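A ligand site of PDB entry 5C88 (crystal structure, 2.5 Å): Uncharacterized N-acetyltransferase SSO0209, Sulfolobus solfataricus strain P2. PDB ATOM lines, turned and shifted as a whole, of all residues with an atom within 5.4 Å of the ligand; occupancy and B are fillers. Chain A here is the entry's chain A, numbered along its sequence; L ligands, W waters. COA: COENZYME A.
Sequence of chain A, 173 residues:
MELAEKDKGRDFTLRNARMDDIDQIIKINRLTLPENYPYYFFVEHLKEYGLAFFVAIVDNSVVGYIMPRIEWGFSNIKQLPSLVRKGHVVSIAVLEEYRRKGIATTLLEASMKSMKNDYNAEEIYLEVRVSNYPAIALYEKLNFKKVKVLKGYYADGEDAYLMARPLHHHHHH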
ATOM      1  N   THR A  32      16.196   2.983  -2.472  1.00  0.00           N
ATOM      2  CA  THR A  32      16.534   1.896  -3.393  1.00  0.00           C
ATOM      3  C   THR A  32      15.336   1.058  -3.849  1.00  0.00           C
ATOM      4  O   THR A  32      15.289   0.619  -5.010  1.00  0.00           O
ATOM      5  CB  THR A  32      17.603   0.972  -2.747  1.00  0.00           C
ATOM      6  OG1 THR A  32      18.880   1.629  -2.752  1.00  0.00           O
ATOM      7  CG2 THR A  32      17.737  -0.320  -3.516  1.00  0.00           C
ATOM      8  N   LEU A  33      14.358   0.893  -2.965  1.00  0.00           N
ATOM      9  CA  LEU A  33      13.352  -0.159  -3.080  1.00  0.00           C
ATOM     10  C   LEU A  33      11.923   0.361  -2.917  1.00  0.00           C
ATOM     11  O   LEU A  33      11.730   1.402  -2.306  1.00  0.00           O
ATOM     12  CB  LEU A  33      13.614  -1.228  -2.005  1.00  0.00           C
ATOM     13  CG  LEU A  33      14.839  -2.120  -2.153  1.00  0.00           C
ATOM     14  CD1 LEU A  33      15.232  -2.675  -0.794  1.00  0.00           C
ATOM     15  CD2 LEU A  33      14.570  -3.246  -3.138  1.00  0.00           C
ATOM     16  N   ILE A  92      17.544  -6.623   0.832  1.00  0.00           N
ATOM     17  CA  ILE A  92      18.958  -6.371   0.642  1.00  0.00           C
ATOM     18  C   ILE A  92      19.149  -5.252  -0.374  1.00  0.00           C
ATOM     19  O   ILE A  92      18.635  -5.296  -1.462  1.00  0.00           O
ATOM     20  CB  ILE A  92      19.743  -7.628   0.187  1.00  0.00           C
ATOM     21  CG1 ILE A  92      21.157  -7.250  -0.227  1.00  0.00           C
ATOM     22  CG2 ILE A  92      19.067  -8.330  -0.984  1.00  0.00           C
ATOM     23  CD1 ILE A  92      21.959  -8.423  -0.719  1.00  0.00           C
ATOM     24  N   ALA A  93      19.905  -4.228   0.006  1.00  0.00           N
ATOM     25  CA  ALA A  93      20.072  -3.091  -0.861  1.00  0.00           C
ATOM     26  C   ALA A  93      21.477  -2.533  -0.747  1.00  0.00           C
ATOM     27  O   ALA A  93      22.081  -2.590   0.321  1.00  0.00           O
ATOM     28  CB  ALA A  93      19.042  -2.036  -0.545  1.00  0.00           C
ATOM     29  N   VAL A  94      21.979  -2.040  -1.871  1.00  0.00           N
ATOM     30  CA  VAL A  94      23.253  -1.330  -1.950  1.00  0.00           C
ATOM     31  C   VAL A  94      23.017  -0.018  -2.647  1.00  0.00           C
ATOM     32  O   VAL A  94      22.350   0.022  -3.680  1.00  0.00           O
ATOM     33  CB  VAL A  94      24.322  -2.116  -2.742  1.00  0.00           C
ATOM     34  CG1 VAL A  94      25.653  -1.344  -2.766  1.00  0.00           C
ATOM     35  CG2 VAL A  94      24.481  -3.541  -2.191  1.00  0.00           C
ATOM     36  N   LEU A  95      23.540   1.072  -2.071  1.00  0.00           N
ATOM     37  CA  LEU A  95      23.431   2.389  -2.693  1.00  0.00           C
ATOM     38  C   LEU A  95      24.056   2.400  -4.102  1.00  0.00           C
ATOM     39  O   LEU A  95      25.176   1.934  -4.301  1.00  0.00           O
ATOM     40  CB  LEU A  95      24.083   3.450  -1.823  1.00  0.00           C
ATOM     41  CG  LEU A  95      23.299   3.954  -0.617  1.00  0.00           C
ATOM     42  CD1 LEU A  95      24.165   4.884   0.215  1.00  0.00           C
ATOM     43  CD2 LEU A  95      22.037   4.649  -1.069  1.00  0.00           C
ATOM     44  N   TYR A  98      27.623   2.680  -5.178  1.00  0.00           N
ATOM     45  CA  TYR A  98      28.598   1.717  -4.679  1.00  0.00           C
ATOM     46  C   TYR A  98      28.423   0.317  -5.253  1.00  0.00           C
ATOM     47  O   TYR A  98      29.079  -0.613  -4.792  1.00  0.00           O
ATOM     48  CB  TYR A  98      28.518   1.691  -3.162  1.00  0.00           C
ATOM     49  CG  TYR A  98      28.767   3.045  -2.547  1.00  0.00           C
ATOM     50  CD1 TYR A  98      30.059   3.513  -2.319  1.00  0.00           C
ATOM     51  CD2 TYR A  98      27.702   3.875  -2.202  1.00  0.00           C
ATOM     52  CE1 TYR A  98      30.279   4.752  -1.755  1.00  0.00           C
ATOM     53  CE2 TYR A  98      27.913   5.117  -1.633  1.00  0.00           C
ATOM     54  CZ  TYR A  98      29.199   5.555  -1.416  1.00  0.00           C
ATOM     55  OH  TYR A  98      29.405   6.790  -0.852  1.00  0.00           O
ATOM     56  N   ARG A  99      27.559   0.176  -6.259  1.00  0.00           N
ATOM     57  CA  ARG A  99      27.268  -1.121  -6.886  1.00  0.00           C
ATOM     58  C   ARG A  99      28.403  -1.654  -7.742  1.00  0.00           C
ATOM     59  O   ARG A  99      29.311  -0.923  -8.123  1.00  0.00           O
ATOM     60  CB  ARG A  99      26.009  -1.000  -7.731  1.00  0.00           C
ATOM     61  CG  ARG A  99      24.891  -0.440  -6.935  1.00  0.00           C
ATOM     62  CD  ARG A  99      23.543  -0.585  -7.566  1.00  0.00           C
ATOM     63  NE  ARG A  99      22.533  -0.200  -6.578  1.00  0.00           N
ATOM     64  CZ  ARG A  99      21.321   0.230  -6.851  1.00  0.00           C
ATOM     65  NH1 ARG A  99      20.915   0.309  -8.115  1.00  0.00           N
ATOM     66  NH2 ARG A  99      20.504   0.567  -5.869  1.00  0.00           N
ATOM     67  N   ARG A 100      28.319  -2.948  -8.047  1.00  0.00           N
ATOM     68  CA  ARG A 100      29.309  -3.642  -8.881  1.00  0.00           C
ATOM     69  C   ARG A 100      30.684  -3.609  -8.268  1.00  0.00           C
ATOM     70  O   ARG A 100      31.681  -3.825  -8.958  1.00  0.00           O
ATOM     71  CB  ARG A 100      29.386  -3.036 -10.287  1.00  0.00           C
ATOM     72  CG  ARG A 100      28.234  -3.324 -11.211  1.00  0.00           C
ATOM     73  CD  ARG A 100      28.520  -2.629 -12.525  1.00  0.00           C
ATOM     74  NE  ARG A 100      27.498  -2.842 -13.539  1.00  0.00           N
ATOM     75  CZ  ARG A 100      27.249  -4.014 -14.122  1.00  0.00           C
ATOM     76  NH1 ARG A 100      27.943  -5.091 -13.789  1.00  0.00           N
ATOM     77  NH2 ARG A 100      26.308  -4.090 -15.050  1.00  0.00           N
ATOM     78  N   LYS A 101      30.753  -3.337  -6.973  1.00  0.00           N
ATOM     79  CA  LYS A 101      32.023  -3.365  -6.276  1.00  0.00           C
ATOM     80  C   LYS A 101      32.111  -4.571  -5.350  1.00  0.00           C
ATOM     81  O   LYS A 101      32.966  -4.617  -4.483  1.00  0.00           O
ATOM     82  CB  LYS A 101      32.246  -2.079  -5.490  1.00  0.00           C
ATOM     83  CG  LYS A 101      32.472  -0.850  -6.369  1.00  0.00           C
ATOM     84  CD  LYS A 101      33.632   0.017  -5.871  1.00  0.00           C
ATOM     85  CE  LYS A 101      34.979  -0.724  -5.914  1.00  0.00           C
ATOM     86  NZ  LYS A 101      36.079   0.028  -5.201  1.00  0.00           N
ATOM     87  N   GLY A 102      31.204  -5.540  -5.530  1.00  0.00           N
ATOM     88  CA  GLY A 102      31.207  -6.766  -4.751  1.00  0.00           C
ATOM     89  C   GLY A 102      30.412  -6.750  -3.435  1.00  0.00           C
ATOM     90  O   GLY A 102      30.426  -7.743  -2.689  1.00  0.00           O
ATOM     91  N   ILE A 103      29.703  -5.668  -3.150  1.00  0.00           N
ATOM     92  CA  ILE A 103      29.057  -5.543  -1.848  1.00  0.00           C
ATOM     93  C   ILE A 103      27.936  -6.581  -1.619  1.00  0.00           C
ATOM     94  O   ILE A 103      27.920  -7.243  -0.582  1.00  0.00           O
ATOM     95  CB  ILE A 103      28.487  -4.143  -1.636  1.00  0.00           C
ATOM     96  CG1 ILE A 103      29.631  -3.124  -1.506  1.00  0.00           C
ATOM     97  CG2 ILE A 103      27.706  -4.089  -0.371  1.00  0.00           C
ATOM     98  CD1 ILE A 103      29.160  -1.692  -1.245  1.00  0.00           C
ATOM     99  N   ALA A 104      27.009  -6.712  -2.568  1.00  0.00           N
ATOM    100  CA  ALA A 104      25.844  -7.568  -2.340  1.00  0.00           C
ATOM    101  C   ALA A 104      26.217  -9.063  -2.272  1.00  0.00           C
ATOM    102  O   ALA A 104      25.544  -9.847  -1.581  1.00  0.00           O
ATOM    103  CB  ALA A 104      24.806  -7.336  -3.390  1.00  0.00           C
ATOM    104  N   THR A 105      27.285  -9.430  -2.954  1.00  0.00           N
ATOM    105  CA  THR A 105      27.821 -10.786  -2.876  1.00  0.00           C
ATOM    106  C   THR A 105      28.347 -11.110  -1.479  1.00  0.00           C
ATOM    107  O   THR A 105      28.136 -12.199  -0.944  1.00  0.00           O
ATOM    108  CB  THR A 105      28.939 -10.976  -3.891  1.00  0.00           C
ATOM    109  OG1 THR A 105      28.386 -10.915  -5.212  1.00  0.00           O
ATOM    110  CG2 THR A 105      29.593 -12.324  -3.708  1.00  0.00           C
ATOM    111  N   THR A 106      29.038 -10.148  -0.892  1.00  0.00           N
ATOM    112  CA  THR A 106      29.641 -10.269   0.437  1.00  0.00           C
ATOM    113  C   THR A 106      28.585 -10.285   1.533  1.00  0.00           C
ATOM    114  O   THR A 106      28.693 -11.061   2.508  1.00  0.00           O
ATOM    115  CB  THR A 106      30.609  -9.106   0.688  1.00  0.00           C
ATOM    116  OG1 THR A 106      31.369  -8.866  -0.516  1.00  0.00           O
ATOM    117  CG2 THR A 106      31.547  -9.416   1.820  1.00  0.00           C
ATOM    118  N   GLU A 127      12.493 -13.670  -2.561  1.00  0.00           N
ATOM    119  CA  GLU A 127      11.640 -13.293  -3.678  1.00  0.00           C
ATOM    120  C   GLU A 127      12.356 -12.217  -4.462  1.00  0.00           C
ATOM    121  O   GLU A 127      12.884 -11.300  -3.872  1.00  0.00           O
ATOM    122  CB  GLU A 127      10.283 -12.781  -3.208  1.00  0.00           C
ATOM    123  CG  GLU A 127       9.370 -13.854  -2.664  1.00  0.00           C
ATOM    124  CD  GLU A 127       9.579 -14.141  -1.186  1.00  0.00           C
ATOM    125  OE1 GLU A 127      10.546 -13.606  -0.616  1.00  0.00           O
ATOM    126  OE2 GLU A 127       8.775 -14.910  -0.619  1.00  0.00           O
ATOM    127  N   VAL A 128      12.367 -12.324  -5.790  1.00  0.00           N
ATOM    128  CA  VAL A 128      12.895 -11.248  -6.609  1.00  0.00           C
ATOM    129  C   VAL A 128      11.977 -11.011  -7.805  1.00  0.00           C
ATOM    130  O   VAL A 128      11.439 -11.950  -8.371  1.00  0.00           O
ATOM    131  CB  VAL A 128      14.353 -11.540  -7.071  1.00  0.00           C
ATOM    132  CG1 VAL A 128      14.424 -12.724  -8.029  1.00  0.00           C
ATOM    133  CG2 VAL A 128      14.931 -10.321  -7.754  1.00  0.00           C
ATOM    134  N   ASN A 132      14.010  -7.773 -12.476  1.00  0.00           N
ATOM    135  CA  ASN A 132      15.218  -7.323 -11.767  1.00  0.00           C
ATOM    136  C   ASN A 132      16.450  -8.112 -12.197  1.00  0.00           C
ATOM    137  O   ASN A 132      17.004  -8.902 -11.422  1.00  0.00           O
ATOM    138  CB  ASN A 132      14.985  -7.468 -10.258  1.00  0.00           C
ATOM    139  CG  ASN A 132      16.063  -6.793  -9.408  1.00  0.00           C
ATOM    140  OD1 ASN A 132      17.164  -6.498  -9.865  1.00  0.00           O
ATOM    141  ND2 ASN A 132      15.750  -6.599  -8.129  1.00  0.00           N
ATOM    142  N   TYR A 133      16.872  -7.908 -13.440  1.00  0.00           N
ATOM    143  CA  TYR A 133      17.965  -8.668 -14.046  1.00  0.00           C
ATOM    144  C   TYR A 133      19.259  -8.720 -13.215  1.00  0.00           C
ATOM    145  O   TYR A 133      19.771  -9.816 -12.959  1.00  0.00           O
ATOM    146  CB  TYR A 133      18.257  -8.114 -15.437  1.00  0.00           C
ATOM    147  CG  TYR A 133      19.395  -8.802 -16.134  1.00  0.00           C
ATOM    148  CD1 TYR A 133      19.234 -10.042 -16.722  1.00  0.00           C
ATOM    149  CD2 TYR A 133      20.642  -8.195 -16.202  1.00  0.00           C
ATOM    150  CE1 TYR A 133      20.292 -10.678 -17.362  1.00  0.00           C
ATOM    151  CE2 TYR A 133      21.704  -8.817 -16.845  1.00  0.00           C
ATOM    152  CZ  TYR A 133      21.527 -10.050 -17.424  1.00  0.00           C
ATOM    153  OH  TYR A 133      22.581 -10.668 -18.063  1.00  0.00           O
ATOM    154  N   PRO A 134      19.790  -7.551 -12.784  1.00  0.00           N
ATOM    155  CA  PRO A 134      21.049  -7.630 -12.022  1.00  0.00           C
ATOM    156  C   PRO A 134      20.945  -8.389 -10.699  1.00  0.00           C
ATOM    157  O   PRO A 134      21.948  -8.973 -10.257  1.00  0.00           O
ATOM    158  CB  PRO A 134      21.399  -6.161 -11.772  1.00  0.00           C
ATOM    159  CG  PRO A 134      20.119  -5.431 -11.917  1.00  0.00           C
ATOM    160  CD  PRO A 134      19.363  -6.149 -12.972  1.00  0.00           C
ATOM    161  N   ALA A 135      19.778  -8.371 -10.052  1.00  0.00           N
ATOM    162  CA  ALA A 135      19.632  -9.179  -8.841  1.00  0.00           C
ATOM    163  C   ALA A 135      19.644 -10.659  -9.197  1.00  0.00           C
ATOM    164  O   ALA A 135      20.415 -11.417  -8.614  1.00  0.00           O
ATOM    165  CB  ALA A 135      18.368  -8.822  -8.108  1.00  0.00           C
ATOM    166  N   ALA A 137      20.851 -12.098 -11.708  1.00  0.00           N
ATOM    167  CA  ALA A 137      22.214 -12.432 -12.084  1.00  0.00           C
ATOM    168  C   ALA A 137      23.111 -12.707 -10.851  1.00  0.00           C
ATOM    169  O   ALA A 137      23.926 -13.632 -10.856  1.00  0.00           O
ATOM    170  CB  ALA A 137      22.815 -11.318 -12.936  1.00  0.00           C
ATOM    171  N   LEU A 138      22.947 -11.911  -9.793  1.00  0.00           N
ATOM    172  CA  LEU A 138      23.756 -12.087  -8.582  1.00  0.00           C
ATOM    173  C   LEU A 138      23.462 -13.402  -7.854  1.00  0.00           C
ATOM    174  O   LEU A 138      24.370 -14.109  -7.420  1.00  0.00           O
ATOM    175  CB  LEU A 138      23.548 -10.905  -7.630  1.00  0.00           C
ATOM    176  CG  LEU A 138      24.315 -10.921  -6.307  1.00  0.00           C
ATOM    177  CD1 LEU A 138      25.075  -9.644  -6.085  1.00  0.00           C
ATOM    178  CD2 LEU A 138      23.347 -11.067  -5.188  1.00  0.00           C
ATOM    179  N   TYR A 139      22.179 -13.743  -7.731  1.00  0.00           N
ATOM    180  CA  TYR A 139      21.773 -14.953  -7.029  1.00  0.00           C
ATOM    181  C   TYR A 139      22.212 -16.215  -7.771  1.00  0.00           C
ATOM    182  O   TYR A 139      22.709 -17.142  -7.152  1.00  0.00           O
ATOM    183  CB  TYR A 139      20.257 -14.963  -6.819  1.00  0.00           C
ATOM    184  CG  TYR A 139      19.751 -13.717  -6.144  1.00  0.00           C
ATOM    185  CD1 TYR A 139      20.424 -13.176  -5.052  1.00  0.00           C
ATOM    186  CD2 TYR A 139      18.624 -13.066  -6.602  1.00  0.00           C
ATOM    187  CE1 TYR A 139      19.967 -12.033  -4.431  1.00  0.00           C
ATOM    188  CE2 TYR A 139      18.158 -11.917  -6.000  1.00  0.00           C
ATOM    189  CZ  TYR A 139      18.831 -11.407  -4.907  1.00  0.00           C
ATOM    190  OH  TYR A 139      18.372 -10.257  -4.293  1.00  0.00           O
ATOM    191  N   LYS A 141      24.641 -16.555  -9.812  1.00  0.00           N
ATOM    192  CA  LYS A 141      26.095 -16.576  -9.673  1.00  0.00           C
ATOM    193  C   LYS A 141      26.487 -17.247  -8.357  1.00  0.00           C
ATOM    194  O   LYS A 141      27.484 -17.967  -8.300  1.00  0.00           O
ATOM    195  CB  LYS A 141      26.653 -15.146  -9.736  1.00  0.00           C
ATOM    196  CG  LYS A 141      28.165 -15.054  -9.931  1.00  0.00           C
ATOM    197  CD  LYS A 141      28.767 -13.898  -9.143  1.00  0.00           C
ATOM    198  CE  LYS A 141      30.303 -14.009  -9.052  1.00  0.00           C
ATOM    199  NZ  LYS A 141      30.891 -13.142  -7.979  1.00  0.00           N
HETATM  200  N1A COA L   1      24.119  -5.492 -14.009  1.00  0.00           N
HETATM  201  C2A COA L   1      24.219  -6.834 -14.267  1.00  0.00           C
HETATM  202  N3A COA L   1      24.582  -7.705 -13.280  1.00  0.00           N
HETATM  203  C4A COA L   1      24.839  -7.243 -12.016  1.00  0.00           C
HETATM  204  C5A COA L   1      24.752  -5.927 -11.756  1.00  0.00           C
HETATM  205  C6A COA L   1      24.389  -5.048 -12.775  1.00  0.00           C
HETATM  206  N6A COA L   1      24.136  -3.685 -13.128  1.00  0.00           N
HETATM  207  N7A COA L   1      25.053  -5.720 -10.448  1.00  0.00           N
HETATM  208  C8A COA L   1      25.343  -6.929  -9.897  1.00  0.00           C
HETATM  209  N9A COA L   1      25.212  -7.875 -10.861  1.00  0.00           N
HETATM  210  C1B COA L   1      25.410  -9.285 -10.734  1.00  0.00           C
HETATM  211  C2B COA L   1      26.444  -9.689 -11.428  1.00  0.00           C
HETATM  212  O2B COA L   1      26.251 -11.055 -11.880  1.00  0.00           O
HETATM  213  C3B COA L   1      27.716  -9.612 -10.423  1.00  0.00           C
HETATM  214  O3B COA L   1      28.720 -10.499 -10.909  1.00  0.00           O
HETATM  215  P3B COA L   1      29.999  -9.876 -11.647  1.00  0.00           P
HETATM  216  O7A COA L   1      31.209 -10.705 -11.298  1.00  0.00           O
HETATM  217  O8A COA L   1      30.168  -8.438 -11.185  1.00  0.00           O
HETATM  218  O9A COA L   1      29.772  -9.936 -13.146  1.00  0.00           O
HETATM  219  C4B COA L   1      27.253 -10.031  -9.218  1.00  0.00           C
HETATM  220  O4B COA L   1      25.802  -9.579  -9.226  1.00  0.00           O
HETATM  221  C5B COA L   1      27.975  -9.403  -8.037  1.00  0.00           C
HETATM  222  O5B COA L   1      27.618  -8.032  -7.923  1.00  0.00           O
HETATM  223  P1A COA L   1      27.839  -7.250  -6.534  1.00  0.00           P
HETATM  224  O1A COA L   1      28.395  -8.182  -5.472  1.00  0.00           O
HETATM  225  O2A COA L   1      28.818  -6.106  -6.731  1.00  0.00           O
HETATM  226  O3A COA L   1      26.411  -6.747  -6.074  1.00  0.00           O
HETATM  227  P2A COA L   1      25.965  -5.260  -6.045  1.00  0.00           P
HETATM  228  O4A COA L   1      26.300  -4.617  -7.383  1.00  0.00           O
HETATM  229  O5A COA L   1      26.696  -4.572  -4.920  1.00  0.00           O
HETATM  230  O6A COA L   1      24.335  -5.135  -5.796  1.00  0.00           O
HETATM  231  CBP COA L   1      22.119  -5.160  -6.985  1.00  0.00           C
HETATM  232  CCP COA L   1      23.412  -5.921  -6.580  1.00  0.00           C
HETATM  233  CDP COA L   1      22.426  -3.807  -7.697  1.00  0.00           C
HETATM  234  CEP COA L   1      21.302  -6.063  -7.933  1.00  0.00           C
HETATM  235  CAP COA L   1      21.246  -4.874  -5.697  1.00  0.00           C
HETATM  236  OAP COA L   1      21.749  -5.640  -4.646  1.00  0.00           O
HETATM  237  C9P COA L   1      21.258  -3.437  -5.327  1.00  0.00           C
HETATM  238  O9P COA L   1      22.149  -2.985  -4.695  1.00  0.00           O
HETATM  239  N8P COA L   1      20.203  -2.520  -5.708  1.00  0.00           N
HETATM  240  C7P COA L   1      19.069  -2.964  -6.489  1.00  0.00           C
HETATM  241  C6P COA L   1      17.857  -3.109  -5.512  1.00  0.00           C
HETATM  242  C5P COA L   1      16.879  -4.141  -6.150  1.00  0.00           C
HETATM  243  O5P COA L   1      16.297  -3.872  -7.191  1.00  0.00           O
HETATM  244  N4P COA L   1      16.686  -5.415  -5.495  1.00  0.00           N
HETATM  245  C3P COA L   1      17.368  -5.697  -4.298  1.00  0.00           C
HETATM  246  C2P COA L   1      16.594  -6.803  -3.530  1.00  0.00           C
HETATM  247  S1P COA L   1      15.708  -7.849  -4.676  1.00  0.00           S
HETATM  248  O   HOH W   1      29.301  -3.215  -4.800  1.00  0.00           O
HETATM  249  O   HOH W   2      13.113  -7.005  -6.811  1.00  0.00           O
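The backbone carbonyl oxygen (O) of Val 94 is in hydrogen-bond range of the guanidinium group (NE) of Arg 99 (2.9 Å).
OD1 of Asn 132 lies close to N of Ala 135, at 3.2 Å.
OG1 of Thr 106 lies within hydrogen-bond range of O of Gly 102.
The side-chain hydroxyl (OH) of Tyr 139 lies close to a sulfur (S1P) of the ligand, at 3.6 Å.
The guanidinium group of Arg 100 is in hydrogen-bond range of a nitrogen (N1A) of the ligand (2.8 Å).
The backbone NH (N) of Val 94 lies within hydrogen-bond range of an oxygen (O9P) of the ligand (3.0 Å).
The guanidinium group (NE) of Arg 99 sits at hydrogen-bond distance from an oxygen (O9P) of the ligand (3.4 Å).
ND2 of Asn 132 is in hydrogen-bond range of O5P of the ligand, at 2.9 Å.
O5A of the ligand is in hydrogen-bond range of N of Ala 104 (3.2 Å).
An oxygen (O1A) of the ligand lies within hydrogen-bond range of the side-chain hydroxyl of Thr 105, at 2.7 Å.
N of Lys 101 lies within hydrogen-bond range of O2A of the ligand, 3.4 Å away.
The backbone NH of Thr 105 is in hydrogen-bond range of an oxygen (O1A) of the ligand (3.0 Å).
O4A of the ligand sits at hydrogen-bond distance from N of Arg 100, 2.7 Å away.
The backbone NH of Gly 102 is in hydrogen-bond range of an oxygen (O2A) of the ligand, 2.7 Å away.
The backbone carbonyl oxygen of Pro 134 lies close to a nitrogen (N9A) of the ligand, at 3.5 Å.
Thr 32 touches the ligand.
CD2 of Leu 33 touches N4P of the ligand (3.8 Å).
Ile 92 touches the ligand.
N of Ile 103 touches O5A of the ligand (3.7 Å).
Ala 135 touches the ligand (N to CEP, 3.5 Å).
Ala 137 touches the ligand.
Leu 138 touches the ligand.
Lys 141 touches the ligand (CD to O3B, 3.8 Å).
Hydrophobic or aromatic side chains that line the ligand: Leu 33, Ile 92, Val 94, Ile 103, Ala 104, Pro 134, Ala 137 and Leu 138.
Water W2 bridges ND2 of Asn 132 (3.0 Å) and S1P of the ligand (3.5 Å).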
